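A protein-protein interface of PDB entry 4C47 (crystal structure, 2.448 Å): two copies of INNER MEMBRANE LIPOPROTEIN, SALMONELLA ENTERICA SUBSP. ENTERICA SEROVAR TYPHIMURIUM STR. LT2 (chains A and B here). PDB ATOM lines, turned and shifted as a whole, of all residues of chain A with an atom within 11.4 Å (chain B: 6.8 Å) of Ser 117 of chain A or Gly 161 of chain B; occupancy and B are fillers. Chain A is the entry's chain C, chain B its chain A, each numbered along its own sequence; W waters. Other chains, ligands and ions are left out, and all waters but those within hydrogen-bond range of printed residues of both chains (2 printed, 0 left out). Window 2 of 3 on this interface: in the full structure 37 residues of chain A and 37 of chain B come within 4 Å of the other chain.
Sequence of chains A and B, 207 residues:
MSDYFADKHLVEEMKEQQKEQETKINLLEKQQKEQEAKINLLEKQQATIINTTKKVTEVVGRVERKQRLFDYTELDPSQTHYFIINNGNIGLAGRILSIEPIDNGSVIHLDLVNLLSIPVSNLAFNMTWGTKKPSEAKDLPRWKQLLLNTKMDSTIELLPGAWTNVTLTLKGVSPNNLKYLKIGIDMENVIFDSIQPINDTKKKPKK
The backbone carbonyl oxygen (O) of Asn 114 of chain B sits at hydrogen-bond distance from the side-chain hydroxyl (OG) of Ser 117 of chain A (2.6 Å).
The backbone carbonyl oxygen (O) of Leu 115 of chain B lies within hydrogen-bond range of the backbone NH (N) of Ser 117 of chain A, 3.1 Å away.
The side-chain hydroxyl of Ser 117 of chain A sits at hydrogen-bond distance from the backbone NH of Gly 161 of chain B (3.2 Å).
Of the 23 printed residues of chain A, 3 touch a printed residue of chain B.
Along chain A the printed residues that touch a printed residue of chain B span positions 116 to 118.
Hydrophobic or aromatic side chains of chain B that line the printed part of chain A: Val 113 and Leu 115.
Among the printed residues, 7 pairs touch across the chains.
Among the printed residues, no Asp or Glu carboxylate lies within 4 Å of a Lys or Arg side-chain nitrogen of the other chain.
Of chain B, only Asn 114 (2.6 Å), Leu 115 (3.1 Å), Leu 116 (3.6 Å) and Gly 161 (3.2 Å) come within 4 Å of Ser 117 of chain A.
Of chain A, only Ser 117 (3.2 Å) comes within 4 Å of Gly 161 of chain B.
Of chain A, only Ile 118 (3.6 Å) comes within 4 Å of Val 113 of chain B.
Pro 160 of chain B touches none of the printed residues of chain A.
Printed residues of chain B within 4 Å of Leu 116 of chain A: Leu 115 (3.8 Å).
Of the printed residues of chain B, Ile 118 of chain A touches Val 113 and Leu 115.
Of the printed residues of chain A, Leu 116 of chain B touches Ser 117 (3.6 Å).
Glu 157 of chain A touches none of the printed residues of chain B.
The nearest residue of chain B that does not touch Ser 117 of chain A is Pro 160 of chain B (4.1 Å).
The backbone NH of Leu 116 of chain B lies within hydrogen-bond range of the side-chain amide oxygen of Asn 114 of chain B.
ND2 of Asn 114 of chain B sits at hydrogen-bond distance from O of Leu 158 of chain B (3.4 Å).
The backbone carbonyl oxygen of Gly 91 of chain B lies within hydrogen-bond range of the backbone NH of Leu 115 of chain B, at 2.9 Å.
The backbone NH (N) of Leu 116 of chain A is in hydrogen-bond range of the side-chain amide oxygen (OD1) of Asn 114 of chain A (2.7 Å).
O of Asn 114 of chain B lies within hydrogen-bond range of N of Gly 161 of chain B, at 3.2 Å.
The side-chain amide nitrogen of Asn 114 of chain A sits at hydrogen-bond distance from the backbone carbonyl oxygen of Ile 118 of chain A (2.5 Å).
Leu 116 of chain A touches Leu 115 of chain B (CA to O, 3.8 Å).
Leu 116 of chain B touches Ser 117 of chain A.
CG2 of Val 113 of chain B touches CG2 of Ile 118 of chain A (3.6 Å).
Ile 118 of chain A touches Leu 115 of chain B.
Leu 116 of chain A touches Leu 115 of chain B, but with the chains exchanged Leu 115 of chain A does not touch Leu 116 of chain B (6.3 Å).
Ser 117 of chain A touches Asn 114 of chain B, but with the chains exchanged Asn 114 of chain A does not touch Ser 117 of chain B (9.7 Å).
Ser 117 of chain A touches Leu 115 of chain B, but with the chains exchanged Leu 115 of chain A does not touch Ser 117 of chain B (6.5 Å).
Ser 117 of chain A touches Leu 116 of chain B, but with the chains exchanged Leu 116 of chain A does not touch Ser 117 of chain B (6.9 Å).
Positions printed for both chains: 91, 113, 114, 115, 116, 117, 158, 159, 160, 161 and 162.
Water W1 lies within hydrogen-bond range of O of Phe 192 of chain A (2.8 Å), NE1 of Trp 163 of chain B (2.9 Å) and OD1 of Asp 193 of chain A (3.3 Å).
Water W2 lies within hydrogen-bond range of O of Leu 115 of chain B (2.9 Å), O of Leu 115 of chain A (3.1 Å) and N of Ser 117 of chain A (3.5 Å).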
ATOM      1  N   ASN A  89     -11.638 -28.924   8.548  1.00  0.00           N
ATOM      2  CA  ASN A  89     -11.040 -27.667   8.979  1.00  0.00           C
ATOM      3  C   ASN A  89     -11.767 -26.483   8.367  1.00  0.00           C
ATOM      4  O   ASN A  89     -12.176 -25.556   9.066  1.00  0.00           O
ATOM      5  CB  ASN A  89      -9.562 -27.603   8.585  1.00  0.00           C
ATOM      6  CG  ASN A  89      -8.700 -28.548   9.391  1.00  0.00           C
ATOM      7  OD1 ASN A  89      -7.603 -28.914   8.972  1.00  0.00           O
ATOM      8  ND2 ASN A  89      -9.196 -28.956  10.551  1.00  0.00           N
ATOM      9  N   ILE A  90     -11.912 -26.530   7.049  1.00  0.00           N
ATOM     10  CA  ILE A  90     -12.555 -25.470   6.296  1.00  0.00           C
ATOM     11  C   ILE A  90     -13.865 -25.968   5.700  1.00  0.00           C
ATOM     12  O   ILE A  90     -13.902 -27.006   5.042  1.00  0.00           O
ATOM     13  CB  ILE A  90     -11.629 -24.957   5.174  1.00  0.00           C
ATOM     14  CG1 ILE A  90     -10.482 -24.142   5.776  1.00  0.00           C
ATOM     15  CG2 ILE A  90     -12.414 -24.135   4.160  1.00  0.00           C
ATOM     16  CD1 ILE A  90      -9.548 -23.543   4.750  1.00  0.00           C
ATOM     17  N   GLY A  91     -14.941 -25.231   5.956  1.00  0.00           N
ATOM     18  CA  GLY A  91     -16.238 -25.546   5.390  1.00  0.00           C
ATOM     19  C   GLY A  91     -16.631 -24.553   4.312  1.00  0.00           C
ATOM     20  O   GLY A  91     -16.583 -23.343   4.518  1.00  0.00           O
ATOM     21  N   LEU A  92     -17.015 -25.074   3.153  1.00  0.00           N
ATOM     22  CA  LEU A  92     -17.455 -24.257   2.033  1.00  0.00           C
ATOM     23  C   LEU A  92     -18.778 -24.780   1.506  1.00  0.00           C
ATOM     24  O   LEU A  92     -19.015 -25.990   1.486  1.00  0.00           O
ATOM     25  CB  LEU A  92     -16.435 -24.303   0.894  1.00  0.00           C
ATOM     26  CG  LEU A  92     -14.991 -23.892   1.167  1.00  0.00           C
ATOM     27  CD1 LEU A  92     -14.165 -24.077  -0.094  1.00  0.00           C
ATOM     28  CD2 LEU A  92     -14.931 -22.454   1.641  1.00  0.00           C
ATOM     29  N   VAL A 113     -18.908 -20.150  -0.983  1.00  0.00           N
ATOM     30  CA  VAL A 113     -19.038 -19.360   0.232  1.00  0.00           C
ATOM     31  C   VAL A 113     -18.366 -20.012   1.442  1.00  0.00           C
ATOM     32  O   VAL A 113     -18.571 -21.198   1.738  1.00  0.00           O
ATOM     33  CB  VAL A 113     -20.512 -19.001   0.547  1.00  0.00           C
ATOM     34  CG1 VAL A 113     -21.348 -20.250   0.761  1.00  0.00           C
ATOM     35  CG2 VAL A 113     -20.584 -18.086   1.757  1.00  0.00           C
ATOM     36  N   ASN A 114     -17.540 -19.214   2.113  1.00  0.00           N
ATOM     37  CA  ASN A 114     -16.854 -19.602   3.335  1.00  0.00           C
ATOM     38  C   ASN A 114     -17.850 -19.666   4.490  1.00  0.00           C
ATOM     39  O   ASN A 114     -18.521 -18.682   4.799  1.00  0.00           O
ATOM     40  CB  ASN A 114     -15.729 -18.594   3.610  1.00  0.00           C
ATOM     41  CG  ASN A 114     -15.052 -18.794   4.955  1.00  0.00           C
ATOM     42  OD1 ASN A 114     -15.287 -19.774   5.659  1.00  0.00           O
ATOM     43  ND2 ASN A 114     -14.187 -17.851   5.312  1.00  0.00           N
ATOM     44  N   LEU A 115     -17.945 -20.834   5.116  1.00  0.00           N
ATOM     45  CA  LEU A 115     -18.914 -21.072   6.181  1.00  0.00           C
ATOM     46  C   LEU A 115     -18.373 -20.654   7.546  1.00  0.00           C
ATOM     47  O   LEU A 115     -19.111 -20.620   8.532  1.00  0.00           O
ATOM     48  CB  LEU A 115     -19.313 -22.550   6.209  1.00  0.00           C
ATOM     49  CG  LEU A 115     -19.911 -23.126   4.922  1.00  0.00           C
ATOM     50  CD1 LEU A 115     -20.218 -24.610   5.088  1.00  0.00           C
ATOM     51  CD2 LEU A 115     -21.158 -22.359   4.511  1.00  0.00           C
ATOM     52  N   LEU A 116     -17.083 -20.338   7.594  1.00  0.00           N
ATOM     53  CA  LEU A 116     -16.433 -19.952   8.842  1.00  0.00           C
ATOM     54  C   LEU A 116     -16.605 -18.458   9.116  1.00  0.00           C
ATOM     55  O   LEU A 116     -17.140 -17.722   8.284  1.00  0.00           O
ATOM     56  CB  LEU A 116     -14.947 -20.314   8.802  1.00  0.00           C
ATOM     57  CG  LEU A 116     -14.579 -21.737   8.371  1.00  0.00           C
ATOM     58  CD1 LEU A 116     -13.074 -21.958   8.477  1.00  0.00           C
ATOM     59  CD2 LEU A 116     -15.340 -22.785   9.178  1.00  0.00           C
ATOM     60  N   SER A 117     -16.147 -18.015  10.285  1.00  0.00           N
ATOM     61  CA  SER A 117     -16.301 -16.623  10.704  1.00  0.00           C
ATOM     62  C   SER A 117     -15.083 -15.767  10.358  1.00  0.00           C
ATOM     63  O   SER A 117     -15.106 -14.552  10.535  1.00  0.00           O
ATOM     64  CB  SER A 117     -16.569 -16.551  12.206  1.00  0.00           C
ATOM     65  OG  SER A 117     -15.456 -17.041  12.935  1.00  0.00           O
ATOM     66  N   ILE A 118     -14.016 -16.409   9.888  1.00  0.00           N
ATOM     67  CA  ILE A 118     -12.824 -15.696   9.430  1.00  0.00           C
ATOM     68  C   ILE A 118     -12.613 -15.930   7.936  1.00  0.00           C
ATOM     69  O   ILE A 118     -13.039 -16.956   7.405  1.00  0.00           O
ATOM     70  CB  ILE A 118     -11.565 -16.119  10.209  1.00  0.00           C
ATOM     71  CG1 ILE A 118     -11.340 -17.630  10.097  1.00  0.00           C
ATOM     72  CG2 ILE A 118     -11.675 -15.697  11.661  1.00  0.00           C
ATOM     73  CD1 ILE A 118     -10.045 -18.102  10.707  1.00  0.00           C
ATOM     74  N   PRO A 119     -11.967 -14.975   7.249  1.00  0.00           N
ATOM     75  CA  PRO A 119     -11.737 -15.132   5.809  1.00  0.00           C
ATOM     76  C   PRO A 119     -10.813 -16.305   5.505  1.00  0.00           C
ATOM     77  O   PRO A 119      -9.993 -16.666   6.345  1.00  0.00           O
ATOM     78  CB  PRO A 119     -11.051 -13.820   5.419  1.00  0.00           C
ATOM     79  CG  PRO A 119     -11.419 -12.855   6.485  1.00  0.00           C
ATOM     80  CD  PRO A 119     -11.507 -13.664   7.739  1.00  0.00           C
ATOM     81  N   VAL A 120     -10.968 -16.909   4.331  1.00  0.00           N
ATOM     82  CA  VAL A 120      -9.990 -17.879   3.843  1.00  0.00           C
ATOM     83  C   VAL A 120      -9.564 -17.503   2.420  1.00  0.00           C
ATOM     84  O   VAL A 120     -10.401 -17.230   1.556  1.00  0.00           O
ATOM     85  CB  VAL A 120     -10.479 -19.353   3.947  1.00  0.00           C
ATOM     86  CG1 VAL A 120     -11.060 -19.631   5.328  1.00  0.00           C
ATOM     87  CG2 VAL A 120     -11.503 -19.683   2.876  1.00  0.00           C
ATOM     88  N   SER A 121      -8.257 -17.453   2.188  1.00  0.00           N
ATOM     89  CA  SER A 121      -7.733 -17.035   0.893  1.00  0.00           C
ATOM     90  C   SER A 121      -6.694 -18.011   0.358  1.00  0.00           C
ATOM     91  O   SER A 121      -6.077 -18.755   1.120  1.00  0.00           O
ATOM     92  CB  SER A 121      -7.133 -15.628   0.985  1.00  0.00           C
ATOM     93  OG  SER A 121      -8.142 -14.659   1.204  1.00  0.00           O
ATOM     94  N   GLU A 157     -10.311 -14.845  -2.723  1.00  0.00           N
ATOM     95  CA  GLU A 157     -10.575 -14.430  -1.354  1.00  0.00           C
ATOM     96  C   GLU A 157     -12.005 -14.782  -0.960  1.00  0.00           C
ATOM     97  O   GLU A 157     -12.963 -14.292  -1.558  1.00  0.00           O
ATOM     98  CB  GLU A 157     -10.348 -12.925  -1.206  1.00  0.00           C
ATOM     99  CG  GLU A 157     -10.608 -12.397   0.188  1.00  0.00           C
ATOM    100  CD  GLU A 157     -10.427 -10.894   0.279  1.00  0.00           C
ATOM    101  OE1 GLU A 157      -9.956 -10.293  -0.707  1.00  0.00           O
ATOM    102  OE2 GLU A 157     -10.758 -10.315   1.333  1.00  0.00           O
ATOM    103  N   LEU A 158     -12.148 -15.637   0.044  1.00  0.00           N
ATOM    104  CA  LEU A 158     -13.469 -16.029   0.515  1.00  0.00           C
ATOM    105  C   LEU A 158     -13.792 -15.399   1.873  1.00  0.00           C
ATOM    106  O   LEU A 158     -13.402 -15.914   2.925  1.00  0.00           O
ATOM    107  CB  LEU A 158     -13.578 -17.553   0.586  1.00  0.00           C
ATOM    108  CG  LEU A 158     -13.384 -18.298  -0.740  1.00  0.00           C
ATOM    109  CD1 LEU A 158     -13.473 -19.800  -0.528  1.00  0.00           C
ATOM    110  CD2 LEU A 158     -14.405 -17.843  -1.770  1.00  0.00           C
ATOM    111  N   LEU A 159     -14.502 -14.277   1.837  1.00  0.00           N
ATOM    112  CA  LEU A 159     -14.916 -13.584   3.049  1.00  0.00           C
ATOM    113  C   LEU A 159     -16.105 -14.304   3.677  1.00  0.00           C
ATOM    114  O   LEU A 159     -16.930 -14.879   2.966  1.00  0.00           O
ATOM    115  CB  LEU A 159     -15.281 -12.135   2.726  1.00  0.00           C
ATOM    116  CG  LEU A 159     -14.112 -11.239   2.306  1.00  0.00           C
ATOM    117  CD1 LEU A 159     -14.567  -9.803   2.071  1.00  0.00           C
ATOM    118  CD2 LEU A 159     -13.008 -11.282   3.353  1.00  0.00           C
ATOM    119  N   PRO A 160     -16.193 -14.278   5.017  1.00  0.00           N
ATOM    120  CA  PRO A 160     -17.231 -15.004   5.760  1.00  0.00           C
ATOM    121  C   PRO A 160     -18.648 -14.680   5.298  1.00  0.00           C
ATOM    122  O   PRO A 160     -19.036 -13.514   5.289  1.00  0.00           O
ATOM    123  CB  PRO A 160     -17.035 -14.512   7.197  1.00  0.00           C
ATOM    124  CG  PRO A 160     -15.616 -14.120   7.265  1.00  0.00           C
ATOM    125  CD  PRO A 160     -15.276 -13.563   5.921  1.00  0.00           C
ATOM    126  N   GLY A 161     -19.398 -15.708   4.913  1.00  0.00           N
ATOM    127  CA  GLY A 161     -20.800 -15.556   4.572  1.00  0.00           C
ATOM    128  C   GLY A 161     -21.069 -14.953   3.209  1.00  0.00           C
ATOM    129  O   GLY A 161     -22.219 -14.687   2.864  1.00  0.00           O
ATOM    130  N   ALA A 162     -20.013 -14.750   2.428  1.00  0.00           N
ATOM    131  CA  ALA A 162     -20.137 -14.078   1.134  1.00  0.00           C
ATOM    132  C   ALA A 162     -20.062 -15.035  -0.048  1.00  0.00           C
ATOM    133  O   ALA A 162     -19.052 -15.711  -0.254  1.00  0.00           O
ATOM    134  CB  ALA A 162     -19.078 -13.008   0.995  1.00  0.00           C
ATOM    135  N   ILE A 191      -4.398 -18.510   3.648  1.00  0.00           N
ATOM    136  CA  ILE A 191      -4.228 -17.416   4.588  1.00  0.00           C
ATOM    137  C   ILE A 191      -5.590 -17.007   5.134  1.00  0.00           C
ATOM    138  O   ILE A 191      -6.522 -16.753   4.371  1.00  0.00           O
ATOM    139  CB  ILE A 191      -3.561 -16.210   3.917  1.00  0.00           C
ATOM    140  CG1 ILE A 191      -2.138 -16.567   3.485  1.00  0.00           C
ATOM    141  CG2 ILE A 191      -3.553 -15.025   4.857  1.00  0.00           C
ATOM    142  CD1 ILE A 191      -1.377 -15.411   2.900  1.00  0.00           C
ATOM    143  N   PHE A 192      -5.709 -16.957   6.457  1.00  0.00           N
ATOM    144  CA  PHE A 192      -6.986 -16.635   7.085  1.00  0.00           C
ATOM    145  C   PHE A 192      -7.208 -15.134   7.248  1.00  0.00           C
ATOM    146  O   PHE A 192      -7.461 -14.648   8.349  1.00  0.00           O
ATOM    147  CB  PHE A 192      -7.142 -17.359   8.423  1.00  0.00           C
ATOM    148  CG  PHE A 192      -7.233 -18.852   8.288  1.00  0.00           C
ATOM    149  CD1 PHE A 192      -8.354 -19.440   7.728  1.00  0.00           C
ATOM    150  CD2 PHE A 192      -6.195 -19.667   8.708  1.00  0.00           C
ATOM    151  CE1 PHE A 192      -8.438 -20.815   7.594  1.00  0.00           C
ATOM    152  CE2 PHE A 192      -6.277 -21.042   8.575  1.00  0.00           C
ATOM    153  CZ  PHE A 192      -7.398 -21.615   8.019  1.00  0.00           C
ATOM    154  N   ASP A 193      -7.120 -14.415   6.135  1.00  0.00           N
ATOM    155  CA  ASP A 193      -7.355 -12.979   6.116  1.00  0.00           C
ATOM    156  C   ASP A 193      -7.557 -12.508   4.679  1.00  0.00           C
ATOM    157  O   ASP A 193      -7.467 -13.300   3.738  1.00  0.00           O
ATOM    158  CB  ASP A 193      -6.184 -12.237   6.768  1.00  0.00           C
ATOM    159  CG  ASP A 193      -6.539 -10.815   7.164  1.00  0.00           C
ATOM    160  OD1 ASP A 193      -7.745 -10.495   7.210  1.00  0.00           O
ATOM    161  OD2 ASP A 193      -5.614 -10.020   7.430  1.00  0.00           O
ATOM    162  N   SER A 194      -7.847 -11.222   4.518  1.00  0.00           N
ATOM    163  CA  SER A 194      -7.969 -10.623   3.198  1.00  0.00           C
ATOM    164  C   SER A 194      -6.615 -10.620   2.501  1.00  0.00           C
ATOM    165  O   SER A 194      -5.582 -10.409   3.138  1.00  0.00           O
ATOM    166  CB  SER A 194      -8.504  -9.196   3.307  1.00  0.00           C
ATOM    167  OG  SER A 194      -9.782  -9.188   3.918  1.00  0.00           O
ATOM    168  N   GLY B  91     -15.288 -25.232  16.620  1.00  0.00           N
ATOM    169  CA  GLY B  91     -14.183 -25.005  15.710  1.00  0.00           C
ATOM    170  C   GLY B  91     -13.403 -23.762  16.091  1.00  0.00           C
ATOM    171  O   GLY B  91     -13.971 -22.684  16.271  1.00  0.00           O
ATOM    172  N   VAL B 113      -9.215 -17.954  17.572  1.00  0.00           N
ATOM    173  CA  VAL B 113     -10.437 -17.367  17.045  1.00  0.00           C
ATOM    174  C   VAL B 113     -11.549 -18.411  16.905  1.00  0.00           C
ATOM    175  O   VAL B 113     -11.322 -19.535  16.429  1.00  0.00           O
ATOM    176  CB  VAL B 113     -10.198 -16.642  15.694  1.00  0.00           C
ATOM    177  CG1 VAL B 113      -9.740 -17.617  14.618  1.00  0.00           C
ATOM    178  CG2 VAL B 113     -11.452 -15.905  15.262  1.00  0.00           C
ATOM    179  N   ASN B 114     -12.740 -18.032  17.362  1.00  0.00           N
ATOM    180  CA  ASN B 114     -13.931 -18.864  17.264  1.00  0.00           C
ATOM    181  C   ASN B 114     -14.463 -18.862  15.835  1.00  0.00           C
ATOM    182  O   ASN B 114     -14.800 -17.811  15.292  1.00  0.00           O
ATOM    183  CB  ASN B 114     -14.990 -18.361  18.250  1.00  0.00           C
ATOM    184  CG  ASN B 114     -16.307 -19.107  18.141  1.00  0.00           C
ATOM    185  OD1 ASN B 114     -16.379 -20.204  17.591  1.00  0.00           O
ATOM    186  ND2 ASN B 114     -17.363 -18.506  18.678  1.00  0.00           N
ATOM    187  N   LEU B 115     -14.530 -20.045  15.231  1.00  0.00           N
ATOM    188  CA  LEU B 115     -14.939 -20.177  13.837  1.00  0.00           C
ATOM    189  C   LEU B 115     -16.454 -20.169  13.685  1.00  0.00           C
ATOM    190  O   LEU B 115     -16.971 -19.997  12.583  1.00  0.00           O
ATOM    191  CB  LEU B 115     -14.366 -21.461  13.235  1.00  0.00           C
ATOM    192  CG  LEU B 115     -12.842 -21.557  13.183  1.00  0.00           C
ATOM    193  CD1 LEU B 115     -12.397 -22.845  12.488  1.00  0.00           C
ATOM    194  CD2 LEU B 115     -12.263 -20.327  12.492  1.00  0.00           C
ATOM    195  N   LEU B 116     -17.160 -20.352  14.797  1.00  0.00           N
ATOM    196  CA  LEU B 116     -18.615 -20.452  14.778  1.00  0.00           C
ATOM    197  C   LEU B 116     -19.268 -19.068  14.765  1.00  0.00           C
ATOM    198  O   LEU B 116     -18.584 -18.045  14.818  1.00  0.00           O
ATOM    199  CB  LEU B 116     -19.103 -21.256  15.982  1.00  0.00           C
ATOM    200  CG  LEU B 116     -18.446 -22.626  16.187  1.00  0.00           C
ATOM    201  CD1 LEU B 116     -19.077 -23.360  17.364  1.00  0.00           C
ATOM    202  CD2 LEU B 116     -18.527 -23.467  14.916  1.00  0.00           C
ATOM    203  N   SER B 117     -20.596 -19.050  14.699  1.00  0.00           N
ATOM    204  CA  SER B 117     -21.355 -17.810  14.584  1.00  0.00           C
ATOM    205  C   SER B 117     -21.880 -17.317  15.932  1.00  0.00           C
ATOM    206  O   SER B 117     -22.470 -16.242  16.016  1.00  0.00           O
ATOM    207  CB  SER B 117     -22.523 -17.996  13.617  1.00  0.00           C
ATOM    208  OG  SER B 117     -23.419 -18.991  14.084  1.00  0.00           O
ATOM    209  N   LEU B 158     -14.521 -16.121  23.666  1.00  0.00           N
ATOM    210  CA  LEU B 158     -14.153 -16.009  22.261  1.00  0.00           C
ATOM    211  C   LEU B 158     -15.352 -15.614  21.407  1.00  0.00           C
ATOM    212  O   LEU B 158     -16.235 -16.431  21.142  1.00  0.00           O
ATOM    213  CB  LEU B 158     -13.555 -17.323  21.758  1.00  0.00           C
ATOM    214  CG  LEU B 158     -12.287 -17.797  22.469  1.00  0.00           C
ATOM    215  CD1 LEU B 158     -11.864 -19.164  21.955  1.00  0.00           C
ATOM    216  CD2 LEU B 158     -11.166 -16.785  22.293  1.00  0.00           C
ATOM    217  N   LEU B 159     -15.383 -14.351  20.988  1.00  0.00           N
ATOM    218  CA  LEU B 159     -16.449 -13.850  20.125  1.00  0.00           C
ATOM    219  C   LEU B 159     -16.220 -14.327  18.695  1.00  0.00           C
ATOM    220  O   LEU B 159     -15.073 -14.516  18.283  1.00  0.00           O
ATOM    221  CB  LEU B 159     -16.509 -12.320  20.176  1.00  0.00           C
ATOM    222  CG  LEU B 159     -17.043 -11.724  21.478  1.00  0.00           C
ATOM    223  CD1 LEU B 159     -17.046 -10.203  21.422  1.00  0.00           C
ATOM    224  CD2 LEU B 159     -18.442 -12.254  21.764  1.00  0.00           C
ATOM    225  N   PRO B 160     -17.310 -14.534  17.934  1.00  0.00           N
ATOM    226  CA  PRO B 160     -17.200 -15.039  16.561  1.00  0.00           C
ATOM    227  C   PRO B 160     -16.346 -14.138  15.675  1.00  0.00           C
ATOM    228  O   PRO B 160     -16.682 -12.971  15.491  1.00  0.00           O
ATOM    229  CB  PRO B 160     -18.648 -15.018  16.060  1.00  0.00           C
ATOM    230  CG  PRO B 160     -19.481 -15.052  17.281  1.00  0.00           C
ATOM    231  CD  PRO B 160     -18.711 -14.306  18.326  1.00  0.00           C
ATOM    232  N   GLY B 161     -15.249 -14.674  15.148  1.00  0.00           N
ATOM    233  CA  GLY B 161     -14.431 -13.958  14.186  1.00  0.00           C
ATOM    234  C   GLY B 161     -13.324 -13.113  14.789  1.00  0.00           C
ATOM    235  O   GLY B 161     -12.490 -12.564  14.066  1.00  0.00           O
ATOM    236  N   ALA B 162     -13.303 -13.017  16.115  1.00  0.00           N
ATOM    237  CA  ALA B 162     -12.351 -12.150  16.802  1.00  0.00           C
ATOM    238  C   ALA B 162     -11.099 -12.882  17.277  1.00  0.00           C
ATOM    239  O   ALA B 162     -11.149 -13.678  18.218  1.00  0.00           O
ATOM    240  CB  ALA B 162     -13.026 -11.440  17.973  1.00  0.00           C
ATOM    241  N   TRP B 163      -9.980 -12.610  16.614  1.00  0.00           N
ATOM    242  CA  TRP B 163      -8.687 -13.116  17.051  1.00  0.00           C
ATOM    243  C   TRP B 163      -8.403 -12.638  18.468  1.00  0.00           C
ATOM    244  O   TRP B 163      -8.401 -11.436  18.734  1.00  0.00           O
ATOM    245  CB  TRP B 163      -7.577 -12.641  16.111  1.00  0.00           C
ATOM    246  CG  TRP B 163      -7.591 -13.303  14.765  1.00  0.00           C
ATOM    247  CD1 TRP B 163      -7.999 -12.753  13.584  1.00  0.00           C
ATOM    248  CD2 TRP B 163      -7.171 -14.641  14.461  1.00  0.00           C
ATOM    249  NE1 TRP B 163      -7.861 -13.668  12.563  1.00  0.00           N
ATOM    250  CE2 TRP B 163      -7.355 -14.833  13.076  1.00  0.00           C
ATOM    251  CE3 TRP B 163      -6.659 -15.694  15.226  1.00  0.00           C
ATOM    252  CZ2 TRP B 163      -7.044 -16.036  12.440  1.00  0.00           C
ATOM    253  CZ3 TRP B 163      -6.348 -16.889  14.591  1.00  0.00           C
ATOM    254  CH2 TRP B 163      -6.544 -17.048  13.213  1.00  0.00           C
HETATM  255  O   HOH W   1      -7.874 -12.360   9.922  1.00  0.00           O
HETATM  256  O   HOH W   2     -19.332 -19.041  11.243  1.00  0.00           O
